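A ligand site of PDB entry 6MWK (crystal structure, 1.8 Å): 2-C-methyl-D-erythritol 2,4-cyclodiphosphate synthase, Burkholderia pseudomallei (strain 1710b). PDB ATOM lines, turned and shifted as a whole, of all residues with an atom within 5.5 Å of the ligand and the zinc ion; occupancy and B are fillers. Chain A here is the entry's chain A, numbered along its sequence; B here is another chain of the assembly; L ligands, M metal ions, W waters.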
ATOM      1  N   TYR A  13       4.351   1.810  -2.512  1.00  0.00           N
ATOM      2  CA  TYR A  13       5.218   0.862  -1.814  1.00  0.00           C
ATOM      3  C   TYR A  13       6.524   0.751  -2.576  1.00  0.00           C
ATOM      4  O   TYR A  13       6.510   0.690  -3.809  1.00  0.00           O
ATOM      5  CB  TYR A  13       4.570  -0.527  -1.743  1.00  0.00           C
ATOM      6  CG  TYR A  13       5.526  -1.628  -1.317  1.00  0.00           C
ATOM      7  CD1 TYR A  13       5.774  -1.847   0.030  1.00  0.00           C
ATOM      8  CD2 TYR A  13       6.189  -2.422  -2.241  1.00  0.00           C
ATOM      9  CE1 TYR A  13       6.630  -2.841   0.443  1.00  0.00           C
ATOM     10  CE2 TYR A  13       7.076  -3.414  -1.826  1.00  0.00           C
ATOM     11  CZ  TYR A  13       7.279  -3.622  -0.477  1.00  0.00           C
ATOM     12  OH  TYR A  13       8.152  -4.591  -0.035  1.00  0.00           O
ATOM     13  N   ASP A  14       7.650   0.689  -1.871  1.00  0.00           N
ATOM     14  CA  ASP A  14       8.892   0.325  -2.545  1.00  0.00           C
ATOM     15  C   ASP A  14       9.845  -0.341  -1.559  1.00  0.00           C
ATOM     16  O   ASP A  14       9.757  -0.125  -0.355  1.00  0.00           O
ATOM     17  CB  ASP A  14       9.535   1.561  -3.175  1.00  0.00           C
ATOM     18  CG  ASP A  14      10.573   1.206  -4.210  1.00  0.00           C
ATOM     19  OD1 ASP A  14      10.566   0.073  -4.730  1.00  0.00           O
ATOM     20  OD2 ASP A  14      11.412   2.070  -4.514  1.00  0.00           O
ATOM     21  N   VAL A  15      10.780  -1.120  -2.094  1.00  0.00           N
ATOM     22  CA  VAL A  15      11.856  -1.701  -1.285  1.00  0.00           C
ATOM     23  C   VAL A  15      13.094  -1.822  -2.160  1.00  0.00           C
ATOM     24  O   VAL A  15      12.994  -2.098  -3.354  1.00  0.00           O
ATOM     25  CB  VAL A  15      11.452  -3.075  -0.683  1.00  0.00           C
ATOM     26  CG1 VAL A  15      11.259  -4.126  -1.790  1.00  0.00           C
ATOM     27  CG2 VAL A  15      12.512  -3.551   0.322  1.00  0.00           C
ATOM     28  N   HIS A  16      14.268  -1.617  -1.554  1.00  0.00           N
ATOM     29  CA  HIS A  16      15.535  -1.861  -2.224  1.00  0.00           C
ATOM     30  C   HIS A  16      16.478  -2.547  -1.261  1.00  0.00           C
ATOM     31  O   HIS A  16      16.446  -2.286  -0.046  1.00  0.00           O
ATOM     32  CB  HIS A  16      16.178  -0.546  -2.715  1.00  0.00           C
ATOM     33  CG  HIS A  16      15.516   0.055  -3.923  1.00  0.00           C
ATOM     34  ND1 HIS A  16      16.009  -0.116  -5.198  1.00  0.00           N
ATOM     35  CD2 HIS A  16      14.417   0.837  -4.032  1.00  0.00           C
ATOM     36  CE1 HIS A  16      15.228   0.533  -6.055  1.00  0.00           C
ATOM     37  NE2 HIS A  16      14.269   1.119  -5.374  1.00  0.00           N
ATOM     38  N   LEU A  38      20.489  -0.518  -3.615  1.00  0.00           N
ATOM     39  CA  LEU A  38      20.785  -1.046  -4.942  1.00  0.00           C
ATOM     40  C   LEU A  38      19.613  -0.818  -5.894  1.00  0.00           C
ATOM     41  O   LEU A  38      18.493  -1.254  -5.613  1.00  0.00           O
ATOM     42  CB  LEU A  38      21.088  -2.541  -4.858  1.00  0.00           C
ATOM     43  CG  LEU A  38      21.282  -3.242  -6.190  1.00  0.00           C
ATOM     44  CD1 LEU A  38      22.630  -2.857  -6.768  1.00  0.00           C
ATOM     45  CD2 LEU A  38      21.165  -4.749  -5.999  1.00  0.00           C
ATOM     46  N   GLY A  39      19.880  -0.170  -7.023  1.00  0.00           N
ATOM     47  CA  GLY A  39      18.828  -0.041  -8.014  1.00  0.00           C
ATOM     48  C   GLY A  39      19.401   0.482  -9.311  1.00  0.00           C
ATOM     49  O   GLY A  39      20.564   0.886  -9.387  1.00  0.00           O
ATOM     50  N   HIS A  40      18.561   0.461 -10.342  1.00  0.00           N
ATOM     51  CA  HIS A  40      18.977   1.020 -11.630  1.00  0.00           C
ATOM     52  C   HIS A  40      19.166   2.528 -11.514  1.00  0.00           C
ATOM     53  O   HIS A  40      20.147   3.081 -12.032  1.00  0.00           O
ATOM     54  CB  HIS A  40      17.933   0.658 -12.689  1.00  0.00           C
ATOM     55  CG  HIS A  40      18.298   1.099 -14.077  1.00  0.00           C
ATOM     56  ND1 HIS A  40      19.399   0.623 -14.747  1.00  0.00           N
ATOM     57  CD2 HIS A  40      17.691   1.982 -14.913  1.00  0.00           C
ATOM     58  CE1 HIS A  40      19.465   1.192 -15.946  1.00  0.00           C
ATOM     59  NE2 HIS A  40      18.439   2.014 -16.069  1.00  0.00           N
ATOM     60  N   SER A  41      18.251   3.200 -10.808  1.00  0.00           N
ATOM     61  CA  SER A  41      18.333   4.637 -10.553  1.00  0.00           C
ATOM     62  C   SER A  41      19.229   4.879  -9.346  1.00  0.00           C
ATOM     63  O   SER A  41      19.983   3.976  -8.948  1.00  0.00           O
ATOM     64  CB  SER A  41      16.942   5.216 -10.319  1.00  0.00           C
ATOM     65  OG  SER A  41      16.377   4.750  -9.081  1.00  0.00           O
ATOM     66  N   ASP A  42      19.152   6.061  -8.741  1.00  0.00           N
ATOM     67  CA  ASP A  42      19.843   6.222  -7.466  1.00  0.00           C
ATOM     68  C   ASP A  42      19.175   5.419  -6.346  1.00  0.00           C
ATOM     69  O   ASP A  42      19.656   5.460  -5.194  1.00  0.00           O
ATOM     70  CB  ASP A  42      19.942   7.715  -7.085  1.00  0.00           C
ATOM     71  CG  ASP A  42      18.596   8.377  -6.812  1.00  0.00           C
ATOM     72  OD1 ASP A  42      17.574   7.680  -6.666  1.00  0.00           O
ATOM     73  OD2 ASP A  42      18.568   9.634  -6.669  1.00  0.00           O
ATOM     74  N   ALA A  43      18.084   4.705  -6.645  1.00  0.00           N
ATOM     75  CA  ALA A  43      17.481   3.734  -5.737  1.00  0.00           C
ATOM     76  C   ALA A  43      16.818   4.376  -4.521  1.00  0.00           C
ATOM     77  O   ALA A  43      16.690   3.734  -3.458  1.00  0.00           O
ATOM     78  CB  ALA A  43      18.502   2.680  -5.280  1.00  0.00           C
ATOM     79  N   ASP A  44      16.349   5.610  -4.659  1.00  0.00           N
ATOM     80  CA  ASP A  44      15.755   6.348  -3.552  1.00  0.00           C
ATOM     81  C   ASP A  44      14.366   5.793  -3.211  1.00  0.00           C
ATOM     82  O   ASP A  44      13.349   6.187  -3.799  1.00  0.00           O
ATOM     83  CB  ASP A  44      15.677   7.835  -3.885  1.00  0.00           C
ATOM     84  CG  ASP A  44      15.320   8.715  -2.677  1.00  0.00           C
ATOM     85  OD1 ASP A  44      14.532   8.267  -1.804  1.00  0.00           O
ATOM     86  OD2 ASP A  44      15.802   9.859  -2.605  1.00  0.00           O
ATOM     87  N   VAL A  45      14.321   4.887  -2.237  1.00  0.00           N
ATOM     88  CA  VAL A  45      13.113   4.085  -1.978  1.00  0.00           C
ATOM     89  C   VAL A  45      11.933   4.973  -1.540  1.00  0.00           C
ATOM     90  O   VAL A  45      10.782   4.717  -1.897  1.00  0.00           O
ATOM     91  CB  VAL A  45      13.444   2.988  -0.954  1.00  0.00           C
ATOM     92  CG1 VAL A  45      13.871   3.573   0.373  1.00  0.00           C
ATOM     93  CG2 VAL A  45      12.319   1.978  -0.764  1.00  0.00           C
ATOM     94  N   HIS A  48      10.503   6.892  -4.575  1.00  0.00           N
ATOM     95  CA  HIS A  48       9.796   6.018  -5.486  1.00  0.00           C
ATOM     96  C   HIS A  48       8.421   5.694  -4.953  1.00  0.00           C
ATOM     97  O   HIS A  48       7.453   5.642  -5.706  1.00  0.00           O
ATOM     98  CB  HIS A  48      10.563   4.717  -5.738  1.00  0.00           C
ATOM     99  CG  HIS A  48      11.890   4.921  -6.401  1.00  0.00           C
ATOM    100  ND1 HIS A  48      12.803   3.898  -6.579  1.00  0.00           N
ATOM    101  CD2 HIS A  48      12.457   6.028  -6.940  1.00  0.00           C
ATOM    102  CE1 HIS A  48      13.882   4.370  -7.173  1.00  0.00           C
ATOM    103  NE2 HIS A  48      13.696   5.663  -7.418  1.00  0.00           N
ATOM    104  N   ASP A  52       4.920   6.590  -6.823  1.00  0.00           N
ATOM    105  CA  ASP A  52       3.866   5.634  -7.144  1.00  0.00           C
ATOM    106  C   ASP A  52       2.522   6.077  -6.552  1.00  0.00           C
ATOM    107  O   ASP A  52       1.474   5.883  -7.185  1.00  0.00           O
ATOM    108  CB  ASP A  52       4.246   4.254  -6.610  1.00  0.00           C
ATOM    109  CG  ASP A  52       4.714   3.307  -7.693  1.00  0.00           C
ATOM    110  OD1 ASP A  52       4.875   3.755  -8.851  1.00  0.00           O
ATOM    111  OD2 ASP A  52       4.885   2.095  -7.415  1.00  0.00           O
ATOM    112  N   ILE A  63       5.482   3.916 -11.520  1.00  0.00           N
ATOM    113  CA  ILE A  63       6.775   4.479 -11.887  1.00  0.00           C
ATOM    114  C   ILE A  63       7.399   3.658 -13.010  1.00  0.00           C
ATOM    115  O   ILE A  63       8.029   4.217 -13.923  1.00  0.00           O
ATOM    116  CB  ILE A  63       7.651   4.589 -10.621  1.00  0.00           C
ATOM    117  CG1 ILE A  63       8.885   5.455 -10.840  1.00  0.00           C
ATOM    118  CG2 ILE A  63       8.035   3.223 -10.115  1.00  0.00           C
ATOM    119  CD1 ILE A  63       9.725   5.645  -9.565  1.00  0.00           C
ATOM    120  N   GLY A  64       7.159   2.338 -13.029  1.00  0.00           N
ATOM    121  CA  GLY A  64       7.673   1.502 -14.106  1.00  0.00           C
ATOM    122  C   GLY A  64       7.081   1.828 -15.461  1.00  0.00           C
ATOM    123  O   GLY A  64       7.757   1.720 -16.477  1.00  0.00           O
ATOM    124  N   PHE A  67       8.848   5.514 -16.236  1.00  0.00           N
ATOM    125  CA  PHE A  67      10.315   5.621 -16.233  1.00  0.00           C
ATOM    126  C   PHE A  67      10.883   4.202 -16.177  1.00  0.00           C
ATOM    127  O   PHE A  67      11.120   3.654 -15.092  1.00  0.00           O
ATOM    128  CB  PHE A  67      10.826   6.440 -15.058  1.00  0.00           C
ATOM    129  CG  PHE A  67      10.096   7.727 -14.828  1.00  0.00           C
ATOM    130  CD1 PHE A  67      10.154   8.756 -15.760  1.00  0.00           C
ATOM    131  CD2 PHE A  67       9.383   7.940 -13.641  1.00  0.00           C
ATOM    132  CE1 PHE A  67       9.503   9.963 -15.531  1.00  0.00           C
ATOM    133  CE2 PHE A  67       8.717   9.132 -13.419  1.00  0.00           C
ATOM    134  CZ  PHE A  67       8.793  10.154 -14.362  1.00  0.00           C
ATOM    135  N   SER A  68      11.136   3.623 -17.345  1.00  0.00           N
ATOM    136  CA  SER A  68      11.519   2.213 -17.445  1.00  0.00           C
ATOM    137  C   SER A  68      12.786   1.896 -16.650  1.00  0.00           C
ATOM    138  O   SER A  68      13.826   2.567 -16.795  1.00  0.00           O
ATOM    139  CB  SER A  68      11.713   1.829 -18.911  1.00  0.00           C
ATOM    140  OG  SER A  68      11.931   0.441 -19.030  1.00  0.00           O
ATOM    141  N   ASP A  69      12.705   0.847 -15.833  1.00  0.00           N
ATOM    142  CA  ASP A  69      13.832   0.333 -15.053  1.00  0.00           C
ATOM    143  C   ASP A  69      14.948  -0.237 -15.911  1.00  0.00           C
ATOM    144  O   ASP A  69      16.020  -0.539 -15.371  1.00  0.00           O
ATOM    145  CB  ASP A  69      13.344  -0.757 -14.092  1.00  0.00           C
ATOM    146  CG  ASP A  69      12.485  -1.802 -14.803  1.00  0.00           C
ATOM    147  OD1 ASP A  69      12.521  -1.879 -16.054  1.00  0.00           O
ATOM    148  OD2 ASP A  69      11.764  -2.551 -14.100  1.00  0.00           O
ATOM    149  N   THR A  70      14.706  -0.427 -17.201  1.00  0.00           N
ATOM    150  CA  THR A  70      15.722  -0.957 -18.102  1.00  0.00           C
ATOM    151  C   THR A  70      16.168   0.064 -19.144  1.00  0.00           C
ATOM    152  O   THR A  70      17.002  -0.255 -19.995  1.00  0.00           O
ATOM    153  CB  THR A  70      15.185  -2.211 -18.806  1.00  0.00           C
ATOM    154  OG1 THR A  70      13.810  -2.004 -19.141  1.00  0.00           O
ATOM    155  CG2 THR A  70      15.310  -3.412 -17.890  1.00  0.00           C
ATOM    156  N   PHE A  74      17.943   6.230 -17.567  1.00  0.00           N
ATOM    157  CA  PHE A  74      17.650   6.350 -16.152  1.00  0.00           C
ATOM    158  C   PHE A  74      18.700   5.700 -15.260  1.00  0.00           C
ATOM    159  O   PHE A  74      18.491   5.627 -14.056  1.00  0.00           O
ATOM    160  CB  PHE A  74      16.266   5.781 -15.849  1.00  0.00           C
ATOM    161  CG  PHE A  74      15.163   6.502 -16.564  1.00  0.00           C
ATOM    162  CD1 PHE A  74      14.951   7.859 -16.371  1.00  0.00           C
ATOM    163  CD2 PHE A  74      14.324   5.822 -17.444  1.00  0.00           C
ATOM    164  CE1 PHE A  74      13.941   8.528 -17.028  1.00  0.00           C
ATOM    165  CE2 PHE A  74      13.308   6.487 -18.109  1.00  0.00           C
ATOM    166  CZ  PHE A  74      13.122   7.839 -17.905  1.00  0.00           C
ATOM    167  N   ALA A  77      19.657   7.622 -12.241  1.00  0.00           N
ATOM    168  CA  ALA A  77      18.794   8.792 -12.307  1.00  0.00           C
ATOM    169  C   ALA A  77      18.562   9.405 -10.929  1.00  0.00           C
ATOM    170  O   ALA A  77      18.372   8.685  -9.937  1.00  0.00           O
ATOM    171  CB  ALA A  77      17.443   8.440 -12.930  1.00  0.00           C
ATOM    172  N   LEU A  82      12.910  12.652 -11.194  1.00  0.00           N
ATOM    173  CA  LEU A  82      11.794  11.797 -11.571  1.00  0.00           C
ATOM    174  C   LEU A  82      10.524  12.179 -10.812  1.00  0.00           C
ATOM    175  O   LEU A  82       9.433  12.213 -11.396  1.00  0.00           O
ATOM    176  CB  LEU A  82      12.156  10.340 -11.297  1.00  0.00           C
ATOM    177  CG  LEU A  82      13.301   9.727 -12.108  1.00  0.00           C
ATOM    178  CD1 LEU A  82      13.459   8.246 -11.701  1.00  0.00           C
ATOM    179  CD2 LEU A  82      13.129   9.875 -13.592  1.00  0.00           C
ATOM    180  N   LYS B 138       4.804  -4.340  -8.835  1.00  0.00           N
ATOM    181  CA  LYS B 138       6.222  -4.225  -8.440  1.00  0.00           C
ATOM    182  C   LYS B 138       6.776  -5.615  -8.139  1.00  0.00           C
ATOM    183  O   LYS B 138       6.022  -6.526  -7.819  1.00  0.00           O
ATOM    184  CB  LYS B 138       6.416  -3.378  -7.170  1.00  0.00           C
ATOM    185  CG  LYS B 138       5.344  -2.343  -6.863  1.00  0.00           C
ATOM    186  CD  LYS B 138       5.372  -1.194  -7.847  1.00  0.00           C
ATOM    187  CE  LYS B 138       6.704  -0.475  -7.834  1.00  0.00           C
ATOM    188  NZ  LYS B 138       6.702   0.563  -8.913  1.00  0.00           N
ATOM    189  N   GLU B 141      12.332  -6.998  -5.146  1.00  0.00           N
ATOM    190  CA  GLU B 141      13.785  -6.927  -5.224  1.00  0.00           C
ATOM    191  C   GLU B 141      14.458  -8.149  -4.591  1.00  0.00           C
ATOM    192  O   GLU B 141      15.492  -8.054  -3.939  1.00  0.00           O
ATOM    193  CB  GLU B 141      14.300  -5.626  -4.604  1.00  0.00           C
ATOM    194  CG  GLU B 141      14.003  -4.405  -5.460  1.00  0.00           C
ATOM    195  CD  GLU B 141      14.760  -4.423  -6.768  1.00  0.00           C
ATOM    196  OE1 GLU B 141      16.006  -4.515  -6.722  1.00  0.00           O
ATOM    197  OE2 GLU B 141      14.126  -4.373  -7.831  1.00  0.00           O
HETATM  198  C1  LIG L   1      10.319  -0.064 -12.267  1.00  0.00           C
HETATM  199  C2  LIG L   1      10.222   0.589  -9.939  1.00  0.00           C
HETATM  200  C3  LIG L   1      10.131   1.317  -7.784  1.00  0.00           C
HETATM  201  C4  LIG L   1      12.145   1.317  -8.818  1.00  0.00           C
HETATM  202  C5  LIG L   1      14.244   2.605 -11.083  1.00  0.00           C
HETATM  203  C6  LIG L   1      14.759   2.443 -12.353  1.00  0.00           C
HETATM  204  C7  LIG L   1      14.472   3.360 -13.327  1.00  0.00           C
HETATM  205  C8  LIG L   1      13.685   4.473 -13.036  1.00  0.00           C
HETATM  206  C9  LIG L   1      13.187   4.629 -11.734  1.00  0.00           C
HETATM  207  C10 LIG L   1      13.478   3.700 -10.755  1.00  0.00           C
HETATM  208  C11 LIG L   1      11.591   0.830  -9.983  1.00  0.00           C
HETATM  209  N1  LIG L   1       9.508   0.828  -8.843  1.00  0.00           N
HETATM  210  N2  LIG L   1      11.421   1.546  -7.722  1.00  0.00           N
HETATM  211  N3  LIG L   1      13.470   1.620  -8.674  1.00  0.00           N
HETATM  212  N4  LIG L   1      13.402   5.377 -14.005  1.00  0.00           N
HETATM  213  O1  LIG L   1       9.593   0.114 -11.018  1.00  0.00           O
HETATM  214  O2  LIG L   1      14.658  -0.024 -10.498  1.00  0.00           O
HETATM  215  O3  LIG L   1      16.050   1.964  -9.228  1.00  0.00           O
HETATM  216  S1  LIG L   1      14.712   1.412  -9.848  1.00  0.00           S
HETATM  217 ZN    ZN M   1      12.574   1.966  -6.161  1.00  0.00          ZN
HETATM  218  O   HOH W   1       7.695   2.309  -5.987  1.00  0.00           O
HETATM  219  O   HOH W   2       6.402   0.079 -11.391  1.00  0.00           O
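Gly 39 touches the ligand (CA to O3, 3.6 Å). Ile 63 touches the ligand. CA of Gly 64 touches C1 of the ligand (3.6 Å). Ser 68 touches the ligand. Asp 69 touches the ligand (OD2 to C1, 3.4 Å). Phe 74 touches the ligand. Leu 82 touches the ligand (CD1 to C9, 3.6 Å). The nearest printed residue that does not touch the ligand is Ala 43 (4.2 Å).
Water W2 lies within hydrogen-bond range of the side-chain amino group of Lys 138 of chain B, the backbone NH of Gly 64 and an oxygen (O1) of the ligand.
Of the 25 residues printed, 3 come within 4 Å of the zinc ion. The nearest printed residue that does not touch the zinc ion is Val 45 (4.7 Å).
A nitrogen (N2) of the ligand binds the zinc ion. The zinc ion is bound by ND1 of His 48. The zinc ion is bound by OD2 of Asp 14 (2.0 Å). The zinc ion is bound by a ring nitrogen (NE2) of His 16. The zinc ion has four donor atoms within binding distance. Slightly farther from the zinc ion lies a nitrogen (N3) of the ligand (2.7 Å).
The backbone NH (N) of Ala 43 sits close to the side-chain hydroxyl (OG) of Ser 41 (3.0 Å). The side-chain carboxylate (OD1) of Asp 69 sits at hydrogen-bond distance from the side-chain hydroxyl (OG1) of Thr 70, 3.3 Å away. A ring nitrogen (NE2) of His 48 lies close to the side-chain hydroxyl (OG) of Ser 41, at 3.3 Å. The side-chain carboxylate (OD1) of Asp 52 lies within hydrogen-bond range of the backbone NH (N) of Ile 63, 2.7 Å away. The backbone carbonyl oxygen of Leu 38 sits at hydrogen-bond distance from a ring nitrogen (ND1) of His 16. The side-chain hydroxyl (OG) of Ser 68 lies within hydrogen-bond range of the side-chain hydroxyl (OG1) of Thr 70. NZ of Lys 138 of chain B is in salt-bridge range of OD2 of Asp 52, 2.8 Å away.
The side-chain hydroxyl of Ser 41 sits at hydrogen-bond distance from an oxygen (O3) of the ligand (2.8 Å). The backbone NH (N) of Ser 41 sits at hydrogen-bond distance from an oxygen (O3) of the ligand. NZ of Lys 138 of chain B is in hydrogen-bond range of N1 of the ligand, at 2.8 Å. O3 of the ligand lies within hydrogen-bond range of N of His 40, at 3.1 Å. N4 of the ligand sits close to O of Phe 67, at 3.1 Å.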
